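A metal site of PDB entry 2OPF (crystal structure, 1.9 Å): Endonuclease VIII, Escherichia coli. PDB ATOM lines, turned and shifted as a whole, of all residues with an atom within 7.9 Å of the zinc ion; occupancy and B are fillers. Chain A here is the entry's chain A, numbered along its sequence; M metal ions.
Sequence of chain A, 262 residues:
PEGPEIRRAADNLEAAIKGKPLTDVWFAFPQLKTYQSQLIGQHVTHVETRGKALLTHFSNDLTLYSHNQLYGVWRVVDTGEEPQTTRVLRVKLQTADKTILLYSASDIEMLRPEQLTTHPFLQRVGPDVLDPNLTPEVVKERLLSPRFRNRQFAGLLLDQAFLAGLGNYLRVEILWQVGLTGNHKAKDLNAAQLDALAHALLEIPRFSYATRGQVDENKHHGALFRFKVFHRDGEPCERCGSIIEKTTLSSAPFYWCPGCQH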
ATOM      1  N   TRP A 176     -15.440  -4.159  18.669  1.00  0.00           N
ATOM      2  CA  TRP A 176     -14.672  -5.392  18.560  1.00  0.00           C
ATOM      3  C   TRP A 176     -15.468  -6.512  19.211  1.00  0.00           C
ATOM      4  O   TRP A 176     -15.579  -7.613  18.663  1.00  0.00           O
ATOM      5  CB  TRP A 176     -13.321  -5.284  19.258  1.00  0.00           C
ATOM      6  CG  TRP A 176     -12.530  -6.576  19.240  1.00  0.00           C
ATOM      7  CD1 TRP A 176     -11.623  -6.982  18.294  1.00  0.00           C
ATOM      8  CD2 TRP A 176     -12.582  -7.630  20.213  1.00  0.00           C
ATOM      9  NE1 TRP A 176     -11.117  -8.221  18.620  1.00  0.00           N
ATOM     10  CE2 TRP A 176     -11.689  -8.635  19.792  1.00  0.00           C
ATOM     11  CE3 TRP A 176     -13.297  -7.810  21.402  1.00  0.00           C
ATOM     12  CZ2 TRP A 176     -11.485  -9.820  20.515  1.00  0.00           C
ATOM     13  CZ3 TRP A 176     -13.107  -9.000  22.127  1.00  0.00           C
ATOM     14  CH2 TRP A 176     -12.203  -9.979  21.683  1.00  0.00           C
ATOM     15  N   VAL A 229      -8.606  -4.404  22.204  1.00  0.00           N
ATOM     16  CA  VAL A 229      -7.986  -3.800  21.027  1.00  0.00           C
ATOM     17  C   VAL A 229      -7.417  -2.406  21.267  1.00  0.00           C
ATOM     18  O   VAL A 229      -6.469  -2.010  20.601  1.00  0.00           O
ATOM     19  CB  VAL A 229      -8.964  -3.697  19.823  1.00  0.00           C
ATOM     20  CG1 VAL A 229      -9.341  -5.074  19.345  1.00  0.00           C
ATOM     21  CG2 VAL A 229     -10.199  -2.898  20.214  1.00  0.00           C
ATOM     22  N   PRO A 236      -1.394  -9.381  18.347  1.00  0.00           N
ATOM     23  CA  PRO A 236      -2.356 -10.385  17.890  1.00  0.00           C
ATOM     24  C   PRO A 236      -3.686 -10.406  18.645  1.00  0.00           C
ATOM     25  O   PRO A 236      -3.724 -10.378  19.877  1.00  0.00           O
ATOM     26  CB  PRO A 236      -1.589 -11.691  18.045  1.00  0.00           C
ATOM     27  CG  PRO A 236      -0.757 -11.433  19.265  1.00  0.00           C
ATOM     28  CD  PRO A 236      -0.256 -10.020  19.029  1.00  0.00           C
ATOM     29  N   CYS A 237      -4.780 -10.445  17.880  1.00  0.00           N
ATOM     30  CA  CYS A 237      -6.132 -10.500  18.424  1.00  0.00           C
ATOM     31  C   CYS A 237      -6.265 -11.744  19.285  1.00  0.00           C
ATOM     32  O   CYS A 237      -5.882 -12.829  18.862  1.00  0.00           O
ATOM     33  CB  CYS A 237      -7.141 -10.539  17.267  1.00  0.00           C
ATOM     34  SG  CYS A 237      -8.881 -10.711  17.734  1.00  0.00           S
ATOM     35  N   GLU A 238      -6.815 -11.603  20.485  1.00  0.00           N
ATOM     36  CA  GLU A 238      -6.961 -12.756  21.353  1.00  0.00           C
ATOM     37  C   GLU A 238      -8.084 -13.683  20.890  1.00  0.00           C
ATOM     38  O   GLU A 238      -8.202 -14.804  21.372  1.00  0.00           O
ATOM     39  CB  GLU A 238      -7.201 -12.330  22.806  1.00  0.00           C
ATOM     40  CG  GLU A 238      -8.525 -11.648  23.064  1.00  0.00           C
ATOM     41  CD  GLU A 238      -8.701 -11.326  24.533  1.00  0.00           C
ATOM     42  OE1 GLU A 238      -7.902 -10.527  25.070  1.00  0.00           O
ATOM     43  OE2 GLU A 238      -9.639 -11.878  25.143  1.00  0.00           O
ATOM     44  N   ARG A 239      -8.901 -13.202  19.960  1.00  0.00           N
ATOM     45  CA  ARG A 239     -10.017 -13.997  19.466  1.00  0.00           C
ATOM     46  C   ARG A 239      -9.663 -14.803  18.212  1.00  0.00           C
ATOM     47  O   ARG A 239      -9.981 -15.997  18.138  1.00  0.00           O
ATOM     48  CB  ARG A 239     -11.211 -13.100  19.163  1.00  0.00           C
ATOM     49  CG  ARG A 239     -12.272 -13.756  18.301  1.00  0.00           C
ATOM     50  CD  ARG A 239     -13.211 -12.700  17.738  1.00  0.00           C
ATOM     51  NE  ARG A 239     -14.137 -12.227  18.743  1.00  0.00           N
ATOM     52  CZ  ARG A 239     -14.710 -11.033  18.742  1.00  0.00           C
ATOM     53  NH1 ARG A 239     -14.450 -10.156  17.780  1.00  0.00           N
ATOM     54  NH2 ARG A 239     -15.568 -10.726  19.706  1.00  0.00           N
ATOM     55  N   CYS A 240      -9.032 -14.157  17.239  1.00  0.00           N
ATOM     56  CA  CYS A 240      -8.688 -14.837  15.992  1.00  0.00           C
ATOM     57  C   CYS A 240      -7.215 -14.836  15.615  1.00  0.00           C
ATOM     58  O   CYS A 240      -6.826 -15.453  14.619  1.00  0.00           O
ATOM     59  CB  CYS A 240      -9.487 -14.226  14.832  1.00  0.00           C
ATOM     60  SG  CYS A 240      -8.871 -12.640  14.193  1.00  0.00           S
ATOM     61  N   GLY A 241      -6.385 -14.138  16.392  1.00  0.00           N
ATOM     62  CA  GLY A 241      -4.962 -14.126  16.097  1.00  0.00           C
ATOM     63  C   GLY A 241      -4.462 -13.122  15.062  1.00  0.00           C
ATOM     64  O   GLY A 241      -3.253 -12.929  14.949  1.00  0.00           O
ATOM     65  N   SER A 242      -5.355 -12.503  14.301  1.00  0.00           N
ATOM     66  CA  SER A 242      -4.935 -11.520  13.302  1.00  0.00           C
ATOM     67  C   SER A 242      -4.280 -10.330  14.012  1.00  0.00           C
ATOM     68  O   SER A 242      -4.487 -10.131  15.208  1.00  0.00           O
ATOM     69  CB  SER A 242      -6.128 -11.027  12.477  1.00  0.00           C
ATOM     70  OG  SER A 242      -6.609 -12.026  11.586  1.00  0.00           O
ATOM     71  N   ILE A 243      -3.512  -9.530  13.274  1.00  0.00           N
ATOM     72  CA  ILE A 243      -2.839  -8.373  13.869  1.00  0.00           C
ATOM     73  C   ILE A 243      -3.739  -7.147  13.927  1.00  0.00           C
ATOM     74  O   ILE A 243      -4.226  -6.675  12.909  1.00  0.00           O
ATOM     75  CB  ILE A 243      -1.553  -8.015  13.087  1.00  0.00           C
ATOM     76  CG1 ILE A 243      -0.599  -9.211  13.081  1.00  0.00           C
ATOM     77  CG2 ILE A 243      -0.885  -6.797  13.725  1.00  0.00           C
ATOM     78  CD1 ILE A 243      -0.237  -9.741  14.466  1.00  0.00           C
ATOM     79  N   ILE A 244      -3.956  -6.630  15.128  1.00  0.00           N
ATOM     80  CA  ILE A 244      -4.802  -5.450  15.316  1.00  0.00           C
ATOM     81  C   ILE A 244      -4.205  -4.245  14.604  1.00  0.00           C
ATOM     82  O   ILE A 244      -2.994  -4.044  14.612  1.00  0.00           O
ATOM     83  CB  ILE A 244      -4.999  -5.105  16.815  1.00  0.00           C
ATOM     84  CG1 ILE A 244      -5.943  -6.121  17.465  1.00  0.00           C
ATOM     85  CG2 ILE A 244      -5.584  -3.705  16.963  1.00  0.00           C
ATOM     86  CD1 ILE A 244      -5.370  -7.501  17.588  1.00  0.00           C
ATOM     87  N   TRP A 256      -8.899  -1.862  15.554  1.00  0.00           N
ATOM     88  CA  TRP A 256      -9.786  -2.947  15.156  1.00  0.00           C
ATOM     89  C   TRP A 256      -9.032  -4.153  14.614  1.00  0.00           C
ATOM     90  O   TRP A 256      -7.853  -4.040  14.256  1.00  0.00           O
ATOM     91  CB  TRP A 256     -10.773  -2.453  14.099  1.00  0.00           C
ATOM     92  CG  TRP A 256     -10.113  -2.141  12.792  1.00  0.00           C
ATOM     93  CD1 TRP A 256      -9.188  -1.154  12.549  1.00  0.00           C
ATOM     94  CD2 TRP A 256     -10.315  -2.808  11.546  1.00  0.00           C
ATOM     95  NE1 TRP A 256      -8.799  -1.183  11.236  1.00  0.00           N
ATOM     96  CE2 TRP A 256      -9.474  -2.189  10.597  1.00  0.00           C
ATOM     97  CE3 TRP A 256     -11.116  -3.881  11.139  1.00  0.00           C
ATOM     98  CZ2 TRP A 256      -9.414  -2.613   9.253  1.00  0.00           C
ATOM     99  CZ3 TRP A 256     -11.059  -4.295   9.810  1.00  0.00           C
ATOM    100  CH2 TRP A 256     -10.212  -3.663   8.895  1.00  0.00           C
ATOM    101  N   CYS A 257      -9.705  -5.292  14.573  1.00  0.00           N
ATOM    102  CA  CYS A 257      -9.096  -6.512  14.045  1.00  0.00           C
ATOM    103  C   CYS A 257      -9.749  -6.847  12.702  1.00  0.00           C
ATOM    104  O   CYS A 257     -10.954  -7.097  12.630  1.00  0.00           O
ATOM    105  CB  CYS A 257      -9.293  -7.686  15.011  1.00  0.00           C
ATOM    106  SG  CYS A 257      -8.603  -9.246  14.343  1.00  0.00           S
ATOM    107  N   PRO A 258      -8.948  -6.861  11.620  1.00  0.00           N
ATOM    108  CA  PRO A 258      -9.450  -7.171  10.284  1.00  0.00           C
ATOM    109  C   PRO A 258      -9.891  -8.626  10.174  1.00  0.00           C
ATOM    110  O   PRO A 258     -10.649  -8.992   9.275  1.00  0.00           O
ATOM    111  CB  PRO A 258      -8.250  -6.875   9.376  1.00  0.00           C
ATOM    112  CG  PRO A 258      -7.439  -5.884  10.180  1.00  0.00           C
ATOM    113  CD  PRO A 258      -7.528  -6.471  11.564  1.00  0.00           C
ATOM    114  N   GLY A 259      -9.412  -9.452  11.096  1.00  0.00           N
ATOM    115  CA  GLY A 259      -9.750 -10.859  11.069  1.00  0.00           C
ATOM    116  C   GLY A 259     -11.099 -11.246  11.637  1.00  0.00           C
ATOM    117  O   GLY A 259     -11.693 -12.249  11.218  1.00  0.00           O
ATOM    118  N   CYS A 260     -11.607 -10.471  12.593  1.00  0.00           N
ATOM    119  CA  CYS A 260     -12.899 -10.805  13.183  1.00  0.00           C
ATOM    120  C   CYS A 260     -13.896  -9.650  13.286  1.00  0.00           C
ATOM    121  O   CYS A 260     -14.954  -9.797  13.896  1.00  0.00           O
ATOM    122  CB  CYS A 260     -12.705 -11.475  14.549  1.00  0.00           C
ATOM    123  SG  CYS A 260     -11.901 -10.489  15.830  1.00  0.00           S
ATOM    124  N   GLN A 261     -13.563  -8.497  12.705  1.00  0.00           N
ATOM    125  CA  GLN A 261     -14.483  -7.372  12.688  1.00  0.00           C
ATOM    126  C   GLN A 261     -14.846  -7.173  11.221  1.00  0.00           C
ATOM    127  O   GLN A 261     -13.980  -6.923  10.379  1.00  0.00           O
ATOM    128  CB  GLN A 261     -13.843  -6.111  13.292  1.00  0.00           C
ATOM    129  CG  GLN A 261     -13.910  -6.113  14.818  1.00  0.00           C
ATOM    130  CD  GLN A 261     -13.265  -4.893  15.465  1.00  0.00           C
ATOM    131  OE1 GLN A 261     -12.083  -4.927  15.818  1.00  0.00           O
ATOM    132  NE2 GLN A 261     -14.029  -3.819  15.604  1.00  0.00           N
ATOM    133  N   HIS A 262     -16.133  -7.310  10.914  1.00  0.00           N
ATOM    134  CA  HIS A 262     -16.618  -7.182   9.538  1.00  0.00           C
ATOM    135  C   HIS A 262     -17.892  -6.355   9.477  1.00  0.00           C
ATOM    136  O   HIS A 262     -18.238  -5.744  10.505  1.00  0.00           O
ATOM    137  CB  HIS A 262     -16.899  -8.574   8.972  1.00  0.00           C
ATOM    138  CG  HIS A 262     -15.731  -9.509   9.086  1.00  0.00           C
ATOM    139  ND1 HIS A 262     -14.659  -9.478   8.228  1.00  0.00           N
ATOM    140  CD2 HIS A 262     -15.456 -10.478  10.000  1.00  0.00           C
ATOM    141  CE1 HIS A 262     -13.771 -10.377   8.594  1.00  0.00           C
ATOM    142  NE2 HIS A 262     -14.232 -11.003   9.665  1.00  0.00           N
ATOM    143  OXT HIS A 262     -18.518  -6.343   8.398  1.00  0.00           O
HETATM  144 ZN    ZN M   1      -9.612 -10.827  15.516  1.00  0.00          ZN
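The side-chain amide oxygen (OE1) of Gln 261 is in hydrogen-bond range of the backbone NH (N) of Cys 257 (2.7 Å).
The backbone NH (N) of Cys 237 lies within hydrogen-bond range of the backbone carbonyl oxygen (O) of Ser 242, at 2.7 Å.
NH1 of Arg 239 sits close to SG of Cys 260 (3.2 Å).
OG of Ser 242 sits close to SG of Cys 240.
SG of Cys 237 lies close to NE1 of Trp 176, 3.5 Å away.
The backbone NH (N) of Arg 239 sits close to the side-chain sulfur (SG) of Cys 237.
The side-chain sulfur (SG) of Cys 257 lies close to the backbone NH (N) of Gly 259 (3.4 Å).
The side-chain sulfur of Cys 260 sits close to the indole nitrogen of Trp 176 (3.7 Å).
The zinc ion is bound by SG of Cys 257 (2.2 Å), SG of Cys 260 (2.3 Å), SG of Cys 237 (2.3 Å) and SG of Cys 240 (2.4 Å).
The zinc ion has four donor atoms within binding distance.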
